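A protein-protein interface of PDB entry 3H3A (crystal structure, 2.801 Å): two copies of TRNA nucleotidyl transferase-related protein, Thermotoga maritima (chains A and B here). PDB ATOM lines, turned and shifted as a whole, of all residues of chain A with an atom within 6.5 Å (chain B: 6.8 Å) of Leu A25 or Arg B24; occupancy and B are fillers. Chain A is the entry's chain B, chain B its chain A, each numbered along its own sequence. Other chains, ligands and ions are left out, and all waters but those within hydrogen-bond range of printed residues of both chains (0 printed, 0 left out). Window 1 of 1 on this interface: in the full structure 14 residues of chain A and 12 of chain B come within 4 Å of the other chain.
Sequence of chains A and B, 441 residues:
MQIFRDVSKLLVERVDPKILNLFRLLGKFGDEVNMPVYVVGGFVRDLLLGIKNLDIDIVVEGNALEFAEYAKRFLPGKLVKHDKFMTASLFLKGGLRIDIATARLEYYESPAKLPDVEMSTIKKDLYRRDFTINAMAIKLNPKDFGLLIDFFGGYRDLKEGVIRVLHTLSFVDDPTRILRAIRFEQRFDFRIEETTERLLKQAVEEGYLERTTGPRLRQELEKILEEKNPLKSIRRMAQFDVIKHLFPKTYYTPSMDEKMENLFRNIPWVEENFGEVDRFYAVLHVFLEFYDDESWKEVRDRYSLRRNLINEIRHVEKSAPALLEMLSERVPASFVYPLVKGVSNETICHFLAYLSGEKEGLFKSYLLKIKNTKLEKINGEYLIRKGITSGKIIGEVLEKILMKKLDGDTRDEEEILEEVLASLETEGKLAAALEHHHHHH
Asn A21 touches Leu B25, and with the chains exchanged Leu A25 touches Asn B21.
Arg A24 touches Leu B25, and with the chains exchanged Leu A25 touches Arg B24.
Arg A24 touches Phe B29, and with the chains exchanged Phe A29 touches Arg B24.
Lys A28 touches Phe B145, and with the chains exchanged Phe A145 touches Lys B28.
The backbone carbonyl oxygen (O) of Pro B17 sits close to the side-chain amide oxygen (OD1) of Asn B21 (3.4 Å).
ND2 of Asn B21 lies close to NH1 of Arg B24, at 3.2 Å.
The backbone carbonyl oxygen (O) of Leu A20 sits close to the guanidinium group (NH1) of Arg A24 (3.5 Å).
OD1 of Asn A21 is in hydrogen-bond range of NH1 of Arg A24, 2.9 Å away.
The side-chain carboxylate (OE1) of Glu A32 is in salt-bridge range of the side-chain amino group (NZ) of Lys A28 (3.3 Å).
OE2 of Glu A32 sits at hydrogen-bond distance from OH of Tyr A70 (2.5 Å).
Of the 17 printed residues of chain B, 7 touch a printed residue of chain A.
Printed residues of chain B that touch a printed residue of chain A: Leu B20, Asn B21, Arg B24, Leu B25, Lys B28, Phe B29 and Phe B145.
Hydrophobic or aromatic side chains of chain B that line the printed part of chain A: Leu B20, Leu B25, Phe B29 and Phe B145.
Of the 17 printed residues of chain A, 9 touch a printed residue of chain B.
Among the printed residues, 15 pairs touch across the chains.
Among the printed residues, Asp or Glu carboxylates within 4 Å of a Lys or Arg side-chain nitrogen of the other chain: Glu A32 with Arg B24.
The side-chain amide oxygen of Asn B21 sits close to the backbone carbonyl oxygen of Phe A74.
The side-chain carboxylate (OE1) of Glu A32 lies within salt-bridge range of the guanidinium group (NE) of Arg B24, at 2.7 Å.
Among the printed residues, merely in contact across the chains: Leu A25 with Asn B21 (3.1 Å), Lys A28 with Phe B145 (3.2 Å), Phe A74 with Arg B24 (3.3 Å), Phe A145 with Lys B28 (3.3 Å), Phe A29 with Arg B24 (3.5 Å), Phe A74 with Leu B20 (3.5 Å), Arg A24 with Phe B29 (3.5 Å), Asn A21 with Leu B25 (3.5 Å), Arg A24 with Leu B25 (3.7 Å), Phe A29 with Asn B21 (3.8 Å), Tyr A70 with Arg B24 (3.9 Å), Lys A28 with Arg B24 (3.97 Å) and Leu A25 with Arg B24 (3.99 Å).
Of the printed residues of chain B, Asn A21 touches Leu B25.
Of the printed residues of chain B, Leu A25 touches Asn B21 and Arg B24.
Of the printed residues of chain B, Phe A29 touches Asn B21 (3.8 Å) and Arg B24 (3.5 Å).
Of the printed residues of chain B, Phe A145 touches Lys B28.
Printed residues of chain A within 4 Å of Arg B24: Leu A25, Lys A28, Phe A29, Glu A32, Tyr A70 and Phe A74.
The nearest printed residue of chain B that does not touch Leu A25 is Leu B25 (4.1 Å).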
ATOM      1  N   LEU A  20      38.218 -26.086 -25.219  1.00  0.00           N
ATOM      2  CA  LEU A  20      37.765 -24.940 -24.450  1.00  0.00           C
ATOM      3  C   LEU A  20      36.563 -24.292 -25.134  1.00  0.00           C
ATOM      4  O   LEU A  20      35.851 -23.485 -24.538  1.00  0.00           O
ATOM      5  CB  LEU A  20      38.910 -23.945 -24.273  1.00  0.00           C
ATOM      6  CG  LEU A  20      38.847 -22.827 -23.229  1.00  0.00           C
ATOM      7  CD1 LEU A  20      38.787 -21.437 -23.858  1.00  0.00           C
ATOM      8  CD2 LEU A  20      37.713 -23.042 -22.266  1.00  0.00           C
ATOM      9  N   ASN A  21      36.339 -24.658 -26.391  1.00  0.00           N
ATOM     10  CA  ASN A  21      35.191 -24.171 -27.137  1.00  0.00           C
ATOM     11  C   ASN A  21      34.007 -25.047 -26.849  1.00  0.00           C
ATOM     12  O   ASN A  21      32.901 -24.564 -26.624  1.00  0.00           O
ATOM     13  CB  ASN A  21      35.463 -24.231 -28.634  1.00  0.00           C
ATOM     14  CG  ASN A  21      35.913 -22.903 -29.206  1.00  0.00           C
ATOM     15  OD1 ASN A  21      36.097 -21.917 -28.485  1.00  0.00           O
ATOM     16  ND2 ASN A  21      36.094 -22.877 -30.521  1.00  0.00           N
ATOM     17  N   LEU A  22      34.258 -26.351 -26.889  1.00  0.00           N
ATOM     18  CA  LEU A  22      33.257 -27.368 -26.607  1.00  0.00           C
ATOM     19  C   LEU A  22      32.697 -27.170 -25.203  1.00  0.00           C
ATOM     20  O   LEU A  22      31.513 -27.366 -24.968  1.00  0.00           O
ATOM     21  CB  LEU A  22      33.884 -28.744 -26.745  1.00  0.00           C
ATOM     22  CG  LEU A  22      32.975 -29.913 -27.053  1.00  0.00           C
ATOM     23  CD1 LEU A  22      32.402 -29.776 -28.446  1.00  0.00           C
ATOM     24  CD2 LEU A  22      33.774 -31.200 -26.938  1.00  0.00           C
ATOM     25  N   PHE A  23      33.549 -26.770 -24.265  1.00  0.00           N
ATOM     26  CA  PHE A  23      33.056 -26.423 -22.941  1.00  0.00           C
ATOM     27  C   PHE A  23      32.063 -25.263 -23.019  1.00  0.00           C
ATOM     28  O   PHE A  23      30.950 -25.366 -22.521  1.00  0.00           O
ATOM     29  CB  PHE A  23      34.199 -26.065 -21.994  1.00  0.00           C
ATOM     30  CG  PHE A  23      34.980 -27.245 -21.520  1.00  0.00           C
ATOM     31  CD1 PHE A  23      34.564 -28.532 -21.819  1.00  0.00           C
ATOM     32  CD2 PHE A  23      36.129 -27.070 -20.763  1.00  0.00           C
ATOM     33  CE1 PHE A  23      35.288 -29.625 -21.381  1.00  0.00           C
ATOM     34  CE2 PHE A  23      36.852 -28.156 -20.322  1.00  0.00           C
ATOM     35  CZ  PHE A  23      36.431 -29.438 -20.628  1.00  0.00           C
ATOM     36  N   ARG A  24      32.474 -24.161 -23.639  1.00  0.00           N
ATOM     37  CA  ARG A  24      31.612 -22.999 -23.801  1.00  0.00           C
ATOM     38  C   ARG A  24      30.286 -23.413 -24.416  1.00  0.00           C
ATOM     39  O   ARG A  24      29.226 -22.970 -23.984  1.00  0.00           O
ATOM     40  CB  ARG A  24      32.273 -21.971 -24.711  1.00  0.00           C
ATOM     41  CG  ARG A  24      33.548 -21.347 -24.176  1.00  0.00           C
ATOM     42  CD  ARG A  24      34.057 -20.346 -25.178  1.00  0.00           C
ATOM     43  NE  ARG A  24      35.155 -19.512 -24.700  1.00  0.00           N
ATOM     44  CZ  ARG A  24      36.404 -19.594 -25.149  1.00  0.00           C
ATOM     45  NH1 ARG A  24      36.720 -20.483 -26.081  1.00  0.00           N
ATOM     46  NH2 ARG A  24      37.333 -18.786 -24.664  1.00  0.00           N
ATOM     47  N   LEU A  25      30.358 -24.272 -25.426  1.00  0.00           N
ATOM     48  CA  LEU A  25      29.168 -24.730 -26.130  1.00  0.00           C
ATOM     49  C   LEU A  25      28.294 -25.636 -25.261  1.00  0.00           C
ATOM     50  O   LEU A  25      27.099 -25.387 -25.113  1.00  0.00           O
ATOM     51  CB  LEU A  25      29.549 -25.440 -27.430  1.00  0.00           C
ATOM     52  CG  LEU A  25      29.995 -24.569 -28.604  1.00  0.00           C
ATOM     53  CD1 LEU A  25      30.246 -25.433 -29.823  1.00  0.00           C
ATOM     54  CD2 LEU A  25      28.950 -23.531 -28.926  1.00  0.00           C
ATOM     55  N   LEU A  26      28.889 -26.690 -24.703  1.00  0.00           N
ATOM     56  CA  LEU A  26      28.180 -27.571 -23.789  1.00  0.00           C
ATOM     57  C   LEU A  26      27.483 -26.769 -22.697  1.00  0.00           C
ATOM     58  O   LEU A  26      26.405 -27.131 -22.254  1.00  0.00           O
ATOM     59  CB  LEU A  26      29.132 -28.588 -23.166  1.00  0.00           C
ATOM     60  CG  LEU A  26      29.518 -29.690 -24.142  1.00  0.00           C
ATOM     61  CD1 LEU A  26      30.648 -30.503 -23.578  1.00  0.00           C
ATOM     62  CD2 LEU A  26      28.319 -30.565 -24.471  1.00  0.00           C
ATOM     63  N   GLY A  27      28.092 -25.670 -22.275  1.00  0.00           N
ATOM     64  CA  GLY A  27      27.514 -24.853 -21.231  1.00  0.00           C
ATOM     65  C   GLY A  27      26.396 -23.964 -21.737  1.00  0.00           C
ATOM     66  O   GLY A  27      25.542 -23.533 -20.971  1.00  0.00           O
ATOM     67  N   LYS A  28      26.398 -23.680 -23.034  1.00  0.00           N
ATOM     68  CA  LYS A  28      25.383 -22.813 -23.615  1.00  0.00           C
ATOM     69  C   LYS A  28      24.159 -23.663 -23.908  1.00  0.00           C
ATOM     70  O   LYS A  28      23.043 -23.270 -23.619  1.00  0.00           O
ATOM     71  CB  LYS A  28      25.908 -22.137 -24.887  1.00  0.00           C
ATOM     72  CG  LYS A  28      25.510 -20.678 -25.034  1.00  0.00           C
ATOM     73  CD  LYS A  28      24.165 -20.531 -25.703  1.00  0.00           C
ATOM     74  CE  LYS A  28      23.495 -19.213 -25.354  1.00  0.00           C
ATOM     75  NZ  LYS A  28      22.092 -19.242 -25.849  1.00  0.00           N
ATOM     76  N   PHE A  29      24.378 -24.845 -24.466  1.00  0.00           N
ATOM     77  CA  PHE A  29      23.319 -25.833 -24.581  1.00  0.00           C
ATOM     78  C   PHE A  29      22.588 -25.987 -23.249  1.00  0.00           C
ATOM     79  O   PHE A  29      21.365 -25.891 -23.180  1.00  0.00           O
ATOM     80  CB  PHE A  29      23.904 -27.185 -24.982  1.00  0.00           C
ATOM     81  CG  PHE A  29      24.639 -27.168 -26.287  1.00  0.00           C
ATOM     82  CD1 PHE A  29      25.478 -28.215 -26.629  1.00  0.00           C
ATOM     83  CD2 PHE A  29      24.497 -26.103 -27.166  1.00  0.00           C
ATOM     84  CE1 PHE A  29      26.149 -28.211 -27.825  1.00  0.00           C
ATOM     85  CE2 PHE A  29      25.169 -26.093 -28.361  1.00  0.00           C
ATOM     86  CZ  PHE A  29      25.997 -27.150 -28.692  1.00  0.00           C
ATOM     87  N   GLY A  30      23.354 -26.240 -22.194  1.00  0.00           N
ATOM     88  CA  GLY A  30      22.815 -26.292 -20.852  1.00  0.00           C
ATOM     89  C   GLY A  30      21.826 -25.175 -20.577  1.00  0.00           C
ATOM     90  O   GLY A  30      20.705 -25.435 -20.151  1.00  0.00           O
ATOM     91  N   GLU A  32      20.295 -23.312 -22.703  1.00  0.00           N
ATOM     92  CA  GLU A  32      19.234 -23.300 -23.704  1.00  0.00           C
ATOM     93  C   GLU A  32      18.204 -24.322 -23.363  1.00  0.00           C
ATOM     94  O   GLU A  32      16.996 -24.079 -23.454  1.00  0.00           O
ATOM     95  CB  GLU A  32      19.790 -23.618 -25.094  1.00  0.00           C
ATOM     96  CG  GLU A  32      20.557 -22.460 -25.737  1.00  0.00           C
ATOM     97  CD  GLU A  32      21.347 -22.892 -26.953  1.00  0.00           C
ATOM     98  OE1 GLU A  32      22.217 -22.104 -27.390  1.00  0.00           O
ATOM     99  OE2 GLU A  32      21.100 -24.017 -27.458  1.00  0.00           O
ATOM    100  N   PHE A  67      19.739 -33.901 -22.975  1.00  0.00           N
ATOM    101  CA  PHE A  67      20.835 -32.969 -23.163  1.00  0.00           C
ATOM    102  C   PHE A  67      21.777 -33.459 -24.251  1.00  0.00           C
ATOM    103  O   PHE A  67      22.263 -32.667 -25.054  1.00  0.00           O
ATOM    104  CB  PHE A  67      21.591 -32.748 -21.850  1.00  0.00           C
ATOM    105  CG  PHE A  67      22.857 -31.970 -22.008  1.00  0.00           C
ATOM    106  CD1 PHE A  67      22.834 -30.586 -22.028  1.00  0.00           C
ATOM    107  CD2 PHE A  67      24.076 -32.622 -22.139  1.00  0.00           C
ATOM    108  CE1 PHE A  67      23.997 -29.862 -22.174  1.00  0.00           C
ATOM    109  CE2 PHE A  67      25.245 -31.907 -22.285  1.00  0.00           C
ATOM    110  CZ  PHE A  67      25.203 -30.523 -22.307  1.00  0.00           C
ATOM    111  N   TYR A  70      20.377 -33.111 -27.761  1.00  0.00           N
ATOM    112  CA  TYR A  70      20.324 -31.695 -28.067  1.00  0.00           C
ATOM    113  C   TYR A  70      21.713 -31.206 -28.446  1.00  0.00           C
ATOM    114  O   TYR A  70      21.868 -30.341 -29.303  1.00  0.00           O
ATOM    115  CB  TYR A  70      19.770 -30.907 -26.887  1.00  0.00           C
ATOM    116  CG  TYR A  70      19.573 -29.453 -27.205  1.00  0.00           C
ATOM    117  CD1 TYR A  70      18.352 -28.977 -27.647  1.00  0.00           C
ATOM    118  CD2 TYR A  70      20.623 -28.556 -27.085  1.00  0.00           C
ATOM    119  CE1 TYR A  70      18.186 -27.631 -27.953  1.00  0.00           C
ATOM    120  CE2 TYR A  70      20.465 -27.220 -27.383  1.00  0.00           C
ATOM    121  CZ  TYR A  70      19.255 -26.761 -27.815  1.00  0.00           C
ATOM    122  OH  TYR A  70      19.122 -25.428 -28.095  1.00  0.00           O
ATOM    123  N   PHE A  74      23.931 -30.227 -32.757  1.00  0.00           N
ATOM    124  CA  PHE A  74      24.885 -29.201 -33.109  1.00  0.00           C
ATOM    125  C   PHE A  74      26.335 -29.658 -32.993  1.00  0.00           C
ATOM    126  O   PHE A  74      27.229 -28.829 -32.975  1.00  0.00           O
ATOM    127  CB  PHE A  74      24.687 -27.980 -32.222  1.00  0.00           C
ATOM    128  CG  PHE A  74      23.272 -27.521 -32.121  1.00  0.00           C
ATOM    129  CD1 PHE A  74      22.456 -27.974 -31.106  1.00  0.00           C
ATOM    130  CD2 PHE A  74      22.764 -26.612 -33.022  1.00  0.00           C
ATOM    131  CE1 PHE A  74      21.156 -27.533 -30.993  1.00  0.00           C
ATOM    132  CE2 PHE A  74      21.463 -26.170 -32.921  1.00  0.00           C
ATOM    133  CZ  PHE A  74      20.655 -26.632 -31.906  1.00  0.00           C
ATOM    134  N   LEU A  75      26.584 -30.957 -32.907  1.00  0.00           N
ATOM    135  CA  LEU A  75      27.963 -31.430 -32.882  1.00  0.00           C
ATOM    136  C   LEU A  75      28.216 -32.500 -33.938  1.00  0.00           C
ATOM    137  O   LEU A  75      27.276 -33.083 -34.466  1.00  0.00           O
ATOM    138  CB  LEU A  75      28.377 -31.910 -31.492  1.00  0.00           C
ATOM    139  CG  LEU A  75      28.471 -30.855 -30.382  1.00  0.00           C
ATOM    140  CD1 LEU A  75      29.036 -31.464 -29.104  1.00  0.00           C
ATOM    141  CD2 LEU A  75      29.312 -29.681 -30.796  1.00  0.00           C
ATOM    142  N   PHE A 145      30.828 -19.551 -15.918  1.00  0.00           N
ATOM    143  CA  PHE A 145      31.752 -20.396 -16.675  1.00  0.00           C
ATOM    144  C   PHE A 145      32.984 -20.850 -15.913  1.00  0.00           C
ATOM    145  O   PHE A 145      33.359 -22.017 -15.951  1.00  0.00           O
ATOM    146  CB  PHE A 145      32.196 -19.715 -17.965  1.00  0.00           C
ATOM    147  CG  PHE A 145      32.994 -20.610 -18.861  1.00  0.00           C
ATOM    148  CD1 PHE A 145      34.309 -20.324 -19.159  1.00  0.00           C
ATOM    149  CD2 PHE A 145      32.428 -21.761 -19.384  1.00  0.00           C
ATOM    150  CE1 PHE A 145      35.048 -21.176 -19.969  1.00  0.00           C
ATOM    151  CE2 PHE A 145      33.158 -22.607 -20.210  1.00  0.00           C
ATOM    152  CZ  PHE A 145      34.467 -22.319 -20.497  1.00  0.00           C
ATOM    153  N   VAL B  12      17.796 -21.322 -33.789  1.00  0.00           N
ATOM    154  CA  VAL B  12      18.229 -22.710 -33.890  1.00  0.00           C
ATOM    155  C   VAL B  12      17.481 -23.427 -34.998  1.00  0.00           C
ATOM    156  O   VAL B  12      18.039 -24.304 -35.659  1.00  0.00           O
ATOM    157  CB  VAL B  12      18.106 -23.514 -32.564  1.00  0.00           C
ATOM    158  CG1 VAL B  12      18.135 -22.584 -31.341  1.00  0.00           C
ATOM    159  CG2 VAL B  12      16.872 -24.394 -32.598  1.00  0.00           C
ATOM    160  N   PRO B  17      23.763 -25.111 -38.062  1.00  0.00           N
ATOM    161  CA  PRO B  17      24.445 -25.342 -36.785  1.00  0.00           C
ATOM    162  C   PRO B  17      25.837 -24.738 -36.755  1.00  0.00           C
ATOM    163  O   PRO B  17      26.211 -24.082 -35.784  1.00  0.00           O
ATOM    164  CB  PRO B  17      24.548 -26.874 -36.708  1.00  0.00           C
ATOM    165  CG  PRO B  17      23.455 -27.371 -37.553  1.00  0.00           C
ATOM    166  CD  PRO B  17      23.334 -26.376 -38.681  1.00  0.00           C
ATOM    167  N   ILE B  19      27.051 -22.300 -38.092  1.00  0.00           N
ATOM    168  CA  ILE B  19      26.907 -20.887 -37.770  1.00  0.00           C
ATOM    169  C   ILE B  19      26.357 -20.582 -36.393  1.00  0.00           C
ATOM    170  O   ILE B  19      26.947 -19.832 -35.642  1.00  0.00           O
ATOM    171  CB  ILE B  19      26.054 -20.200 -38.777  1.00  0.00           C
ATOM    172  CG1 ILE B  19      26.423 -20.699 -40.156  1.00  0.00           C
ATOM    173  CG2 ILE B  19      26.292 -18.737 -38.716  1.00  0.00           C
ATOM    174  CD1 ILE B  19      25.344 -20.476 -41.161  1.00  0.00           C
ATOM    175  N   LEU B  20      25.253 -21.218 -36.032  1.00  0.00           N
ATOM    176  CA  LEU B  20      24.726 -21.040 -34.678  1.00  0.00           C
ATOM    177  C   LEU B  20      25.853 -21.114 -33.665  1.00  0.00           C
ATOM    178  O   LEU B  20      25.995 -20.237 -32.807  1.00  0.00           O
ATOM    179  CB  LEU B  20      23.680 -22.091 -34.333  1.00  0.00           C
ATOM    180  CG  LEU B  20      22.248 -21.625 -34.065  1.00  0.00           C
ATOM    181  CD1 LEU B  20      21.539 -22.683 -33.241  1.00  0.00           C
ATOM    182  CD2 LEU B  20      22.201 -20.281 -33.354  1.00  0.00           C
ATOM    183  N   ASN B  21      26.661 -22.164 -33.770  1.00  0.00           N
ATOM    184  CA  ASN B  21      27.769 -22.337 -32.845  1.00  0.00           C
ATOM    185  C   ASN B  21      28.694 -21.121 -32.859  1.00  0.00           C
ATOM    186  O   ASN B  21      29.345 -20.795 -31.859  1.00  0.00           O
ATOM    187  CB  ASN B  21      28.523 -23.641 -33.129  1.00  0.00           C
ATOM    188  CG  ASN B  21      27.797 -24.871 -32.577  1.00  0.00           C
ATOM    189  OD1 ASN B  21      27.596 -25.854 -33.284  1.00  0.00           O
ATOM    190  ND2 ASN B  21      27.396 -24.808 -31.308  1.00  0.00           N
ATOM    191  N   LEU B  22      28.733 -20.436 -33.995  1.00  0.00           N
ATOM    192  CA  LEU B  22      29.529 -19.228 -34.114  1.00  0.00           C
ATOM    193  C   LEU B  22      28.909 -18.098 -33.330  1.00  0.00           C
ATOM    194  O   LEU B  22      29.576 -17.481 -32.500  1.00  0.00           O
ATOM    195  CB  LEU B  22      29.711 -18.837 -35.577  1.00  0.00           C
ATOM    196  CG  LEU B  22      31.119 -19.150 -36.063  1.00  0.00           C
ATOM    197  CD1 LEU B  22      31.095 -19.905 -37.374  1.00  0.00           C
ATOM    198  CD2 LEU B  22      31.915 -17.855 -36.165  1.00  0.00           C
ATOM    199  N   PHE B  23      27.631 -17.830 -33.589  1.00  0.00           N
ATOM    200  CA  PHE B  23      26.924 -16.808 -32.837  1.00  0.00           C
ATOM    201  C   PHE B  23      27.055 -17.139 -31.354  1.00  0.00           C
ATOM    202  O   PHE B  23      27.414 -16.279 -30.551  1.00  0.00           O
ATOM    203  CB  PHE B  23      25.451 -16.731 -33.228  1.00  0.00           C
ATOM    204  CG  PHE B  23      25.211 -16.301 -34.643  1.00  0.00           C
ATOM    205  CD1 PHE B  23      25.638 -15.067 -35.091  1.00  0.00           C
ATOM    206  CD2 PHE B  23      24.522 -17.121 -35.517  1.00  0.00           C
ATOM    207  CE1 PHE B  23      25.407 -14.665 -36.401  1.00  0.00           C
ATOM    208  CE2 PHE B  23      24.289 -16.729 -36.819  1.00  0.00           C
ATOM    209  CZ  PHE B  23      24.735 -15.498 -37.263  1.00  0.00           C
ATOM    210  N   ARG B  24      26.786 -18.392 -30.993  1.00  0.00           N
ATOM    211  CA  ARG B  24      26.877 -18.813 -29.593  1.00  0.00           C
ATOM    212  C   ARG B  24      28.249 -18.484 -29.042  1.00  0.00           C
ATOM    213  O   ARG B  24      28.375 -17.919 -27.955  1.00  0.00           O
ATOM    214  CB  ARG B  24      26.647 -20.316 -29.458  1.00  0.00           C
ATOM    215  CG  ARG B  24      25.199 -20.752 -29.529  1.00  0.00           C
ATOM    216  CD  ARG B  24      25.121 -22.258 -29.475  1.00  0.00           C
ATOM    217  NE  ARG B  24      23.757 -22.758 -29.539  1.00  0.00           N
ATOM    218  CZ  ARG B  24      23.354 -23.723 -30.356  1.00  0.00           C
ATOM    219  NH1 ARG B  24      24.221 -24.305 -31.178  1.00  0.00           N
ATOM    220  NH2 ARG B  24      22.087 -24.116 -30.330  1.00  0.00           N
ATOM    221  N   LEU B  25      29.277 -18.853 -29.802  1.00  0.00           N
ATOM    222  CA  LEU B  25      30.653 -18.676 -29.369  1.00  0.00           C
ATOM    223  C   LEU B  25      31.032 -17.201 -29.306  1.00  0.00           C
ATOM    224  O   LEU B  25      31.602 -16.731 -28.309  1.00  0.00           O
ATOM    225  CB  LEU B  25      31.593 -19.453 -30.287  1.00  0.00           C
ATOM    226  CG  LEU B  25      31.921 -20.880 -29.838  1.00  0.00           C
ATOM    227  CD1 LEU B  25      32.693 -21.639 -30.894  1.00  0.00           C
ATOM    228  CD2 LEU B  25      32.718 -20.857 -28.556  1.00  0.00           C
ATOM    229  N   LEU B  26      30.701 -16.467 -30.365  1.00  0.00           N
ATOM    230  CA  LEU B  26      31.030 -15.046 -30.436  1.00  0.00           C
ATOM    231  C   LEU B  26      30.431 -14.330 -29.250  1.00  0.00           C
ATOM    232  O   LEU B  26      31.030 -13.421 -28.680  1.00  0.00           O
ATOM    233  CB  LEU B  26      30.499 -14.432 -31.732  1.00  0.00           C
ATOM    234  CG  LEU B  26      31.389 -14.692 -32.945  1.00  0.00           C
ATOM    235  CD1 LEU B  26      30.628 -14.426 -34.201  1.00  0.00           C
ATOM    236  CD2 LEU B  26      32.644 -13.846 -32.879  1.00  0.00           C
ATOM    237  N   GLY B  27      29.235 -14.764 -28.879  1.00  0.00           N
ATOM    238  CA  GLY B  27      28.542 -14.185 -27.751  1.00  0.00           C
ATOM    239  C   GLY B  27      29.303 -14.429 -26.473  1.00  0.00           C
ATOM    240  O   GLY B  27      29.555 -13.494 -25.707  1.00  0.00           O
ATOM    241  N   LYS B  28      29.672 -15.687 -26.241  1.00  0.00           N
ATOM    242  CA  LYS B  28      30.452 -16.000 -25.060  1.00  0.00           C
ATOM    243  C   LYS B  28      31.737 -15.148 -25.047  1.00  0.00           C
ATOM    244  O   LYS B  28      32.068 -14.549 -24.014  1.00  0.00           O
ATOM    245  CB  LYS B  28      30.735 -17.502 -24.954  1.00  0.00           C
ATOM    246  CG  LYS B  28      30.640 -18.072 -23.515  1.00  0.00           C
ATOM    247  CD  LYS B  28      31.669 -17.452 -22.599  1.00  0.00           C
ATOM    248  CE  LYS B  28      31.738 -18.128 -21.243  1.00  0.00           C
ATOM    249  NZ  LYS B  28      32.878 -17.577 -20.394  1.00  0.00           N
ATOM    250  N   PHE B  29      32.436 -15.051 -26.187  1.00  0.00           N
ATOM    251  CA  PHE B  29      33.654 -14.230 -26.245  1.00  0.00           C
ATOM    252  C   PHE B  29      33.324 -12.816 -25.839  1.00  0.00           C
ATOM    253  O   PHE B  29      34.128 -12.150 -25.201  1.00  0.00           O
ATOM    254  CB  PHE B  29      34.270 -14.172 -27.640  1.00  0.00           C
ATOM    255  CG  PHE B  29      34.632 -15.496 -28.205  1.00  0.00           C
ATOM    256  CD1 PHE B  29      34.742 -15.658 -29.575  1.00  0.00           C
ATOM    257  CD2 PHE B  29      34.847 -16.585 -27.378  1.00  0.00           C
ATOM    258  CE1 PHE B  29      35.067 -16.879 -30.111  1.00  0.00           C
ATOM    259  CE2 PHE B  29      35.164 -17.810 -27.906  1.00  0.00           C
ATOM    260  CZ  PHE B  29      35.278 -17.957 -29.278  1.00  0.00           C
ATOM    261  N   LEU B 140      23.829 -11.354 -28.732  1.00  0.00           N
ATOM    262  CA  LEU B 140      24.461 -12.665 -28.822  1.00  0.00           C
ATOM    263  C   LEU B 140      24.996 -13.160 -27.486  1.00  0.00           C
ATOM    264  O   LEU B 140      25.174 -14.360 -27.296  1.00  0.00           O
ATOM    265  CB  LEU B 140      25.580 -12.636 -29.851  1.00  0.00           C
ATOM    266  CG  LEU B 140      25.106 -12.664 -31.297  1.00  0.00           C
ATOM    267  CD1 LEU B 140      26.225 -13.100 -32.219  1.00  0.00           C
ATOM    268  CD2 LEU B 140      23.920 -13.598 -31.441  1.00  0.00           C
ATOM    269  N   ASN B 141      25.251 -12.244 -26.560  1.00  0.00           N
ATOM    270  CA  ASN B 141      25.714 -12.649 -25.247  1.00  0.00           C
ATOM    271  C   ASN B 141      24.713 -13.586 -24.595  1.00  0.00           C
ATOM    272  O   ASN B 141      23.518 -13.357 -24.656  1.00  0.00           O
ATOM    273  CB  ASN B 141      25.959 -11.436 -24.369  1.00  0.00           C
ATOM    274  CG  ASN B 141      26.666 -10.323 -25.104  1.00  0.00           C
ATOM    275  OD1 ASN B 141      27.760  -9.905 -24.717  1.00  0.00           O
ATOM    276  ND2 ASN B 141      26.053  -9.840 -26.179  1.00  0.00           N
ATOM    277  N   PRO B 142      25.203 -14.655 -23.972  1.00  0.00           N
ATOM    278  CA  PRO B 142      24.373 -15.762 -23.494  1.00  0.00           C
ATOM    279  C   PRO B 142      23.185 -15.308 -22.659  1.00  0.00           C
ATOM    280  O   PRO B 142      22.097 -15.864 -22.772  1.00  0.00           O
ATOM    281  CB  PRO B 142      25.344 -16.554 -22.638  1.00  0.00           C
ATOM    282  CG  PRO B 142      26.683 -16.270 -23.233  1.00  0.00           C
ATOM    283  CD  PRO B 142      26.628 -14.855 -23.665  1.00  0.00           C
ATOM    284  N   PHE B 145      20.866 -13.988 -25.333  1.00  0.00           N
ATOM    285  CA  PHE B 145      21.159 -14.587 -26.642  1.00  0.00           C
ATOM    286  C   PHE B 145      20.156 -14.318 -27.785  1.00  0.00           C
ATOM    287  O   PHE B 145      20.495 -13.658 -28.758  1.00  0.00           O
ATOM    288  CB  PHE B 145      21.565 -16.079 -26.516  1.00  0.00           C
ATOM    289  CG  PHE B 145      21.814 -16.760 -27.833  1.00  0.00           C
ATOM    290  CD1 PHE B 145      20.831 -17.538 -28.424  1.00  0.00           C
ATOM    291  CD2 PHE B 145      23.025 -16.608 -28.489  1.00  0.00           C
ATOM    292  CE1 PHE B 145      21.056 -18.158 -29.635  1.00  0.00           C
ATOM    293  CE2 PHE B 145      23.252 -17.227 -29.701  1.00  0.00           C
ATOM    294  CZ  PHE B 145      22.264 -18.005 -30.272  1.00  0.00           C
